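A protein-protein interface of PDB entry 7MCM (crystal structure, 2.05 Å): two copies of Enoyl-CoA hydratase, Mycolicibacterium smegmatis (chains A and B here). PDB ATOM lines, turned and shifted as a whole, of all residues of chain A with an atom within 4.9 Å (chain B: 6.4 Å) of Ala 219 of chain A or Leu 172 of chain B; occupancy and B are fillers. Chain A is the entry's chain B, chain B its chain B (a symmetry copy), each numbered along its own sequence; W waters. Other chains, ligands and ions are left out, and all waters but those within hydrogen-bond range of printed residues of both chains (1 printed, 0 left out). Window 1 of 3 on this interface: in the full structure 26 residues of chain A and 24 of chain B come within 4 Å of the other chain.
NH2 of Arg 207 of chain A lies within hydrogen-bond range of OG1 of Thr 173 of chain B (3.5 Å). OD1 of Asn 211 of chain A sits close to O of Thr 173 of chain B (3.1 Å). The side-chain carboxylate (OE2) of Glu 169 of chain B lies within salt-bridge range of the guanidinium group (NH1) of Arg 207 of chain A, at 3.1 Å. The guanidinium group (NE) of Arg 207 of chain A lies within salt-bridge range of the side-chain carboxylate (OD2) of Asp 175 of chain B (2.8 Å). OD1 of Asn 211 of chain A lies close to O of Leu 172 of chain B (3.0 Å).
N of Asp 175 of chain B lies within hydrogen-bond range of OG1 of Thr 173 of chain B, at 3.1 Å. The side-chain hydroxyl (OG1) of Thr 173 of chain B lies within hydrogen-bond range of the backbone carbonyl oxygen (O) of Glu 169 of chain B (2.7 Å). The side-chain amide oxygen (OD1) of Asn 211 of chain A sits close to the backbone carbonyl oxygen (O) of Ile 208 of chain A (3.4 Å). The side-chain amide oxygen of Asn 211 of chain A sits close to the backbone carbonyl oxygen of Arg 207 of chain A (3.4 Å).
Pro 108 of chain A touches Leu 172 of chain B (CG to CD1, 3.7 Å). Ile 208 of chain A touches Leu 172 of chain B. CG1 of Ile 208 of chain A touches CG2 of Thr 173 of chain B (3.6 Å). Asn 211 of chain A touches Val 144 of chain B (OD1 to CG1, 3.7 Å). Ala 215 of chain A touches Ile 149 of chain B (O to CG2, 3.9 Å). Val 144 of chain B touches Val 216 of chain A. Leu 172 of chain B touches Val 216 of chain A. CB of Met 218 of chain A touches CG2 of Ile 149 of chain B, at 3.7 Å. N of Ala 219 of chain A touches CG2 of Ile 149 of chain B (3.5 Å). Leu 223 of chain A touches Ala 168 of chain B.
Of chain B, only Ile 149 (3.5 Å) and Leu 172 (3.9 Å) come within 4 Å of Ala 219 of chain A. Of the printed residues of chain B, Ala 215 of chain A touches Ile 149 (3.9 Å). Printed residues of chain B within 4 Å of Leu 223 of chain A: Ala 168 (3.9 Å). Of the printed residues of chain B, Leu 222 of chain A touches Ile 149 (3.7 Å). Of the printed residues of chain A, Asp 175 of chain B touches Arg 207 (2.8 Å). Printed residues of chain B within 4 Å of Pro 108 of chain A: Leu 172 (3.7 Å). Ala 167 of chain B touches none of the printed residues of chain A. Thr 171 of chain B touches none of the printed residues of chain A. The nearest printed residue of chain A that does not touch Leu 172 of chain B is Lys 220 of chain A (4.01 Å). The nearest printed residue of chain A that does not touch Asp 175 of chain B is Asn 211 of chain A (5.8 Å).
Of the 15 printed residues of chain B, 7 touch a printed residue of chain A. Hydrophobic or aromatic side chains of chain B within 4 Å of the printed part of chain A: Val 144, Ile 149 and Leu 172. Among the printed residues, 17 pairs touch across the chains. Among the printed residues, Asp or Glu carboxylates within 4 Å of a Lys or Arg side-chain nitrogen of the other chain: Arg 207 of chain A with Glu 169 of chain B (3.1 Å) and Arg 207 of chain A with Asp 175 of chain B (2.8 Å).
No position is printed for both chains.
Water W1 lies within hydrogen-bond range of NH2 of Arg 207 of chain A (2.7 Å) and OE2 of Glu 169 of chain B (3.0 Å).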
ATOM      1  N   PRO A 108      22.462  13.452 -11.449  1.00  0.00           N
ATOM      2  CA  PRO A 108      23.248  13.796 -10.257  1.00  0.00           C
ATOM      3  C   PRO A 108      24.269  14.884 -10.559  1.00  0.00           C
ATOM      4  O   PRO A 108      24.862  14.920 -11.641  1.00  0.00           O
ATOM      5  CB  PRO A 108      23.940  12.481  -9.890  1.00  0.00           C
ATOM      6  CG  PRO A 108      23.263  11.416 -10.674  1.00  0.00           C
ATOM      7  CD  PRO A 108      22.528  12.028 -11.802  1.00  0.00           C
ATOM      8  N   ARG A 207      32.093   6.408 -11.404  1.00  0.00           N
ATOM      9  CA  ARG A 207      31.463   5.347 -10.617  1.00  0.00           C
ATOM     10  C   ARG A 207      29.943   5.383 -10.747  1.00  0.00           C
ATOM     11  O   ARG A 207      29.280   4.356 -10.550  1.00  0.00           O
ATOM     12  CB  ARG A 207      31.866   5.451  -9.144  1.00  0.00           C
ATOM     13  CG  ARG A 207      33.309   5.070  -8.799  1.00  0.00           C
ATOM     14  CD  ARG A 207      33.592   5.475  -7.314  1.00  0.00           C
ATOM     15  NE  ARG A 207      32.638   4.858  -6.398  1.00  0.00           N
ATOM     16  CZ  ARG A 207      32.362   5.285  -5.172  1.00  0.00           C
ATOM     17  NH1 ARG A 207      32.941   6.359  -4.665  1.00  0.00           N
ATOM     18  NH2 ARG A 207      31.485   4.609  -4.433  1.00  0.00           N
ATOM     19  N   ILE A 208      29.382   6.551 -11.047  1.00  0.00           N
ATOM     20  CA  ILE A 208      27.965   6.691 -11.368  1.00  0.00           C
ATOM     21  C   ILE A 208      27.696   6.407 -12.837  1.00  0.00           C
ATOM     22  O   ILE A 208      26.801   5.629 -13.176  1.00  0.00           O
ATOM     23  CB  ILE A 208      27.478   8.103 -10.996  1.00  0.00           C
ATOM     24  CG1 ILE A 208      27.623   8.345  -9.494  1.00  0.00           C
ATOM     25  CG2 ILE A 208      26.050   8.337 -11.481  1.00  0.00           C
ATOM     26  CD1 ILE A 208      27.333   9.785  -9.103  1.00  0.00           C
ATOM     27  N   ASN A 211      26.837   3.051 -14.846  1.00  0.00           N
ATOM     28  CA  ASN A 211      25.565   2.374 -14.672  1.00  0.00           C
ATOM     29  C   ASN A 211      24.568   2.788 -15.743  1.00  0.00           C
ATOM     30  O   ASN A 211      24.689   3.859 -16.333  1.00  0.00           O
ATOM     31  CB  ASN A 211      25.011   2.677 -13.275  1.00  0.00           C
ATOM     32  CG  ASN A 211      25.928   2.180 -12.187  1.00  0.00           C
ATOM     33  OD1 ASN A 211      26.251   2.892 -11.219  1.00  0.00           O
ATOM     34  ND2 ASN A 211      26.383   0.957 -12.350  1.00  0.00           N
ATOM     35  N   ALA A 215      18.411   4.151 -15.223  1.00  0.00           N
ATOM     36  CA  ALA A 215      18.314   3.773 -13.813  1.00  0.00           C
ATOM     37  C   ALA A 215      18.942   4.829 -12.909  1.00  0.00           C
ATOM     38  O   ALA A 215      18.441   5.090 -11.807  1.00  0.00           O
ATOM     39  CB  ALA A 215      18.964   2.415 -13.578  1.00  0.00           C
ATOM     40  N   VAL A 216      20.055   5.427 -13.341  1.00  0.00           N
ATOM     41  CA  VAL A 216      20.660   6.511 -12.568  1.00  0.00           C
ATOM     42  C   VAL A 216      19.661   7.652 -12.356  1.00  0.00           C
ATOM     43  O   VAL A 216      19.527   8.190 -11.245  1.00  0.00           O
ATOM     44  CB  VAL A 216      21.953   6.989 -13.259  1.00  0.00           C
ATOM     45  CG1 VAL A 216      22.413   8.327 -12.667  1.00  0.00           C
ATOM     46  CG2 VAL A 216      23.044   5.932 -13.079  1.00  0.00           C
ATOM     47  N   ARG A 217      18.923   8.018 -13.406  1.00  0.00           N
ATOM     48  CA  ARG A 217      17.986   9.130 -13.291  1.00  0.00           C
ATOM     49  C   ARG A 217      16.775   8.762 -12.444  1.00  0.00           C
ATOM     50  O   ARG A 217      16.258   9.602 -11.697  1.00  0.00           O
ATOM     51  CB  ARG A 217      17.556   9.586 -14.678  1.00  0.00           C
ATOM     52  CG  ARG A 217      18.660  10.375 -15.359  1.00  0.00           C
ATOM     53  CD  ARG A 217      18.229  10.781 -16.731  1.00  0.00           C
ATOM     54  NE  ARG A 217      19.269  11.511 -17.441  1.00  0.00           N
ATOM     55  CZ  ARG A 217      19.024  12.514 -18.263  1.00  0.00           C
ATOM     56  NH1 ARG A 217      17.797  12.978 -18.438  1.00  0.00           N
ATOM     57  NH2 ARG A 217      20.033  13.064 -18.930  1.00  0.00           N
ATOM     58  N   MET A 218      16.285   7.529 -12.583  1.00  0.00           N
ATOM     59  CA  MET A 218      15.170   7.082 -11.758  1.00  0.00           C
ATOM     60  C   MET A 218      15.569   7.032 -10.291  1.00  0.00           C
ATOM     61  O   MET A 218      14.781   7.402  -9.415  1.00  0.00           O
ATOM     62  CB  MET A 218      14.693   5.709 -12.226  1.00  0.00           C
ATOM     63  CG  MET A 218      13.833   5.751 -13.486  1.00  0.00           C
ATOM     64  SD  MET A 218      12.929   4.219 -13.849  1.00  0.00           S
ATOM     65  CE  MET A 218      14.205   2.946 -13.742  1.00  0.00           C
ATOM     66  N   ALA A 219      16.781   6.554 -10.005  1.00  0.00           N
ATOM     67  CA  ALA A 219      17.256   6.516  -8.624  1.00  0.00           C
ATOM     68  C   ALA A 219      17.344   7.916  -8.025  1.00  0.00           C
ATOM     69  O   ALA A 219      16.978   8.121  -6.863  1.00  0.00           O
ATOM     70  CB  ALA A 219      18.616   5.826  -8.546  1.00  0.00           C
ATOM     71  N   LYS A 220      17.854   8.888  -8.785  1.00  0.00           N
ATOM     72  CA  LYS A 220      17.916  10.250  -8.258  1.00  0.00           C
ATOM     73  C   LYS A 220      16.518  10.797  -7.999  1.00  0.00           C
ATOM     74  O   LYS A 220      16.287  11.473  -6.993  1.00  0.00           O
ATOM     75  CB  LYS A 220      18.668  11.182  -9.198  1.00  0.00           C
ATOM     76  CG  LYS A 220      18.446  12.628  -8.747  1.00  0.00           C
ATOM     77  CD  LYS A 220      19.440  13.588  -9.257  1.00  0.00           C
ATOM     78  CE  LYS A 220      19.165  14.972  -8.670  1.00  0.00           C
ATOM     79  NZ  LYS A 220      20.116  15.943  -9.248  1.00  0.00           N
ATOM     80  N   ARG A 221      15.578  10.524  -8.909  1.00  0.00           N
ATOM     81  CA  ARG A 221      14.193  10.938  -8.705  1.00  0.00           C
ATOM     82  C   ARG A 221      13.620  10.317  -7.440  1.00  0.00           C
ATOM     83  O   ARG A 221      12.882  10.970  -6.698  1.00  0.00           O
ATOM     84  CB  ARG A 221      13.353  10.553  -9.924  1.00  0.00           C
ATOM     85  CG  ARG A 221      11.870  10.903  -9.822  1.00  0.00           C
ATOM     86  CD  ARG A 221      11.620  12.407  -9.608  1.00  0.00           C
ATOM     87  NE  ARG A 221      11.245  12.685  -8.223  1.00  0.00           N
ATOM     88  CZ  ARG A 221      10.418  13.649  -7.840  1.00  0.00           C
ATOM     89  NH1 ARG A 221       9.869  14.478  -8.713  1.00  0.00           N
ATOM     90  NH2 ARG A 221      10.123  13.777  -6.549  1.00  0.00           N
ATOM     91  N   LEU A 222      13.939   9.047  -7.188  1.00  0.00           N
ATOM     92  CA  LEU A 222      13.518   8.406  -5.949  1.00  0.00           C
ATOM     93  C   LEU A 222      14.186   9.044  -4.742  1.00  0.00           C
ATOM     94  O   LEU A 222      13.532   9.281  -3.720  1.00  0.00           O
ATOM     95  CB  LEU A 222      13.845   6.918  -6.006  1.00  0.00           C
ATOM     96  CG  LEU A 222      12.671   6.004  -6.270  1.00  0.00           C
ATOM     97  CD1 LEU A 222      13.103   4.549  -6.072  1.00  0.00           C
ATOM     98  CD2 LEU A 222      11.490   6.358  -5.397  1.00  0.00           C
ATOM     99  N   LEU A 223      15.493   9.321  -4.829  1.00  0.00           N
ATOM    100  CA  LEU A 223      16.176   9.977  -3.712  1.00  0.00           C
ATOM    101  C   LEU A 223      15.591  11.357  -3.425  1.00  0.00           C
ATOM    102  O   LEU A 223      15.470  11.750  -2.258  1.00  0.00           O
ATOM    103  CB  LEU A 223      17.672  10.092  -3.988  1.00  0.00           C
ATOM    104  CG  LEU A 223      18.450   8.786  -3.818  1.00  0.00           C
ATOM    105  CD1 LEU A 223      19.771   8.885  -4.548  1.00  0.00           C
ATOM    106  CD2 LEU A 223      18.655   8.508  -2.349  1.00  0.00           C
ATOM    107  N   GLU B 141      23.916  -1.184  -2.110  1.00  0.00           N
ATOM    108  CA  GLU B 141      22.672  -0.754  -2.738  1.00  0.00           C
ATOM    109  C   GLU B 141      22.828  -0.988  -4.241  1.00  0.00           C
ATOM    110  O   GLU B 141      22.969  -0.063  -5.039  1.00  0.00           O
ATOM    111  CB  GLU B 141      22.407   0.713  -2.406  1.00  0.00           C
ATOM    112  CG  GLU B 141      20.999   1.205  -2.662  1.00  0.00           C
ATOM    113  CD  GLU B 141      20.011   0.705  -1.602  1.00  0.00           C
ATOM    114  OE1 GLU B 141      19.938  -0.518  -1.406  1.00  0.00           O
ATOM    115  OE2 GLU B 141      19.290   1.529  -1.005  1.00  0.00           O
ATOM    116  N   VAL B 144      21.086  -0.207  -9.003  1.00  0.00           N
ATOM    117  CA  VAL B 144      21.387   0.616 -10.177  1.00  0.00           C
ATOM    118  C   VAL B 144      22.317  -0.100 -11.146  1.00  0.00           C
ATOM    119  O   VAL B 144      22.267   0.146 -12.364  1.00  0.00           O
ATOM    120  CB  VAL B 144      21.966   1.970  -9.723  1.00  0.00           C
ATOM    121  CG1 VAL B 144      23.371   1.786  -9.135  1.00  0.00           C
ATOM    122  CG2 VAL B 144      21.973   2.964 -10.874  1.00  0.00           C
ATOM    123  N   LEU B 148      18.082  -1.266 -12.194  1.00  0.00           N
ATOM    124  CA  LEU B 148      16.902  -1.277 -11.335  1.00  0.00           C
ATOM    125  C   LEU B 148      17.019  -0.145 -10.330  1.00  0.00           C
ATOM    126  O   LEU B 148      18.080   0.465 -10.193  1.00  0.00           O
ATOM    127  CB  LEU B 148      16.773  -2.611 -10.582  1.00  0.00           C
ATOM    128  CG  LEU B 148      16.765  -3.873 -11.456  1.00  0.00           C
ATOM    129  CD1 LEU B 148      16.894  -5.120 -10.603  1.00  0.00           C
ATOM    130  CD2 LEU B 148      15.485  -3.921 -12.274  1.00  0.00           C
ATOM    131  N   ILE B 149      15.919   0.133  -9.625  1.00  0.00           N
ATOM    132  CA  ILE B 149      15.953   1.043  -8.479  1.00  0.00           C
ATOM    133  C   ILE B 149      15.555   0.239  -7.247  1.00  0.00           C
ATOM    134  O   ILE B 149      15.035  -0.878  -7.389  1.00  0.00           O
ATOM    135  CB  ILE B 149      15.064   2.290  -8.683  1.00  0.00           C
ATOM    136  CG1 ILE B 149      13.648   1.957  -9.186  1.00  0.00           C
ATOM    137  CG2 ILE B 149      15.728   3.248  -9.661  1.00  0.00           C
ATOM    138  CD1 ILE B 149      12.657   1.489  -8.118  1.00  0.00           C
ATOM    139  N   PRO B 150      15.791   0.743  -6.017  1.00  0.00           N
ATOM    140  CA  PRO B 150      15.356  -0.005  -4.830  1.00  0.00           C
ATOM    141  C   PRO B 150      13.836  -0.009  -4.707  1.00  0.00           C
ATOM    142  O   PRO B 150      13.235   0.976  -4.263  1.00  0.00           O
ATOM    143  CB  PRO B 150      16.028   0.744  -3.672  1.00  0.00           C
ATOM    144  CG  PRO B 150      17.133   1.585  -4.324  1.00  0.00           C
ATOM    145  CD  PRO B 150      16.585   1.936  -5.662  1.00  0.00           C
ATOM    146  N   THR B 155      15.422   3.708  -0.588  1.00  0.00           N
ATOM    147  CA  THR B 155      15.814   5.108  -0.746  1.00  0.00           C
ATOM    148  C   THR B 155      15.230   6.006   0.346  1.00  0.00           C
ATOM    149  O   THR B 155      15.730   7.115   0.541  1.00  0.00           O
ATOM    150  CB  THR B 155      15.385   5.655  -2.102  1.00  0.00           C
ATOM    151  OG1 THR B 155      13.966   5.552  -2.207  1.00  0.00           O
ATOM    152  CG2 THR B 155      16.041   4.870  -3.240  1.00  0.00           C
ATOM    153  N   ALA B 167      24.047   8.456   0.982  1.00  0.00           N
ATOM    154  CA  ALA B 167      23.009   7.618   0.388  1.00  0.00           C
ATOM    155  C   ALA B 167      22.998   7.763  -1.132  1.00  0.00           C
ATOM    156  O   ALA B 167      22.758   6.792  -1.855  1.00  0.00           O
ATOM    157  CB  ALA B 167      21.642   7.974   0.968  1.00  0.00           C
ATOM    158  N   ALA B 168      23.223   8.984  -1.623  1.00  0.00           N
ATOM    159  CA  ALA B 168      23.335   9.211  -3.056  1.00  0.00           C
ATOM    160  C   ALA B 168      24.528   8.452  -3.624  1.00  0.00           C
ATOM    161  O   ALA B 168      24.414   7.767  -4.644  1.00  0.00           O
ATOM    162  CB  ALA B 168      23.457  10.716  -3.343  1.00  0.00           C
ATOM    163  N   GLU B 169      25.679   8.542  -2.955  1.00  0.00           N
ATOM    164  CA  GLU B 169      26.848   7.800  -3.408  1.00  0.00           C
ATOM    165  C   GLU B 169      26.558   6.303  -3.485  1.00  0.00           C
ATOM    166  O   GLU B 169      26.851   5.656  -4.496  1.00  0.00           O
ATOM    167  CB  GLU B 169      28.040   8.068  -2.490  1.00  0.00           C
ATOM    168  CG  GLU B 169      29.260   7.250  -2.869  1.00  0.00           C
ATOM    169  CD  GLU B 169      30.429   7.496  -1.953  1.00  0.00           C
ATOM    170  OE1 GLU B 169      30.357   8.441  -1.145  1.00  0.00           O
ATOM    171  OE2 GLU B 169      31.423   6.752  -2.042  1.00  0.00           O
ATOM    172  N   MET B 170      25.957   5.732  -2.434  1.00  0.00           N
ATOM    173  CA  MET B 170      25.697   4.292  -2.454  1.00  0.00           C
ATOM    174  C   MET B 170      24.665   3.926  -3.512  1.00  0.00           C
ATOM    175  O   MET B 170      24.788   2.892  -4.180  1.00  0.00           O
ATOM    176  CB  MET B 170      25.206   3.812  -1.082  1.00  0.00           C
ATOM    177  CG  MET B 170      26.240   3.882   0.023  1.00  0.00           C
ATOM    178  SD  MET B 170      25.603   3.361   1.629  1.00  0.00           S
ATOM    179  CE  MET B 170      25.200   1.658   1.301  1.00  0.00           C
ATOM    180  N   THR B 171      23.620   4.738  -3.655  1.00  0.00           N
ATOM    181  CA  THR B 171      22.525   4.381  -4.549  1.00  0.00           C
ATOM    182  C   THR B 171      22.880   4.620  -6.010  1.00  0.00           C
ATOM    183  O   THR B 171      22.449   3.866  -6.891  1.00  0.00           O
ATOM    184  CB  THR B 171      21.270   5.177  -4.180  1.00  0.00           C
ATOM    185  OG1 THR B 171      21.031   5.055  -2.770  1.00  0.00           O
ATOM    186  CG2 THR B 171      20.070   4.635  -4.936  1.00  0.00           C
ATOM    187  N   LEU B 172      23.654   5.663  -6.293  1.00  0.00           N
ATOM    188  CA  LEU B 172      23.939   6.012  -7.678  1.00  0.00           C
ATOM    189  C   LEU B 172      25.149   5.284  -8.236  1.00  0.00           C
ATOM    190  O   LEU B 172      25.266   5.152  -9.467  1.00  0.00           O
ATOM    191  CB  LEU B 172      24.149   7.529  -7.811  1.00  0.00           C
ATOM    192  CG  LEU B 172      22.981   8.411  -7.334  1.00  0.00           C
ATOM    193  CD1 LEU B 172      23.390   9.894  -7.332  1.00  0.00           C
ATOM    194  CD2 LEU B 172      21.764   8.188  -8.219  1.00  0.00           C
ATOM    195  N   THR B 173      26.076   4.852  -7.384  1.00  0.00           N
ATOM    196  CA  THR B 173      27.159   3.998  -7.866  1.00  0.00           C
ATOM    197  C   THR B 173      26.833   2.518  -7.716  1.00  0.00           C
ATOM    198  O   THR B 173      27.260   1.711  -8.549  1.00  0.00           O
ATOM    199  CB  THR B 173      28.468   4.302  -7.123  1.00  0.00           C
ATOM    200  OG1 THR B 173      28.389   3.830  -5.764  1.00  0.00           O
ATOM    201  CG2 THR B 173      28.756   5.812  -7.143  1.00  0.00           C
ATOM    202  N   GLY B 174      26.083   2.155  -6.679  1.00  0.00           N
ATOM    203  CA  GLY B 174      25.826   0.771  -6.351  1.00  0.00           C
ATOM    204  C   GLY B 174      26.999   0.033  -5.761  1.00  0.00           C
ATOM    205  O   GLY B 174      26.923  -1.192  -5.593  1.00  0.00           O
ATOM    206  N   ASP B 175      28.087   0.726  -5.442  1.00  0.00           N
ATOM    207  CA  ASP B 175      29.309   0.028  -5.072  1.00  0.00           C
ATOM    208  C   ASP B 175      29.234  -0.491  -3.635  1.00  0.00           C
ATOM    209  O   ASP B 175      28.461  -0.010  -2.804  1.00  0.00           O
ATOM    210  CB  ASP B 175      30.515   0.954  -5.216  1.00  0.00           C
ATOM    211  CG  ASP B 175      30.762   1.360  -6.642  1.00  0.00           C
ATOM    212  OD1 ASP B 175      30.232   0.697  -7.563  1.00  0.00           O
ATOM    213  OD2 ASP B 175      31.500   2.345  -6.849  1.00  0.00           O
HETATM  214  O   HOH W   1      31.137   3.760  -1.875  1.00  0.00           O
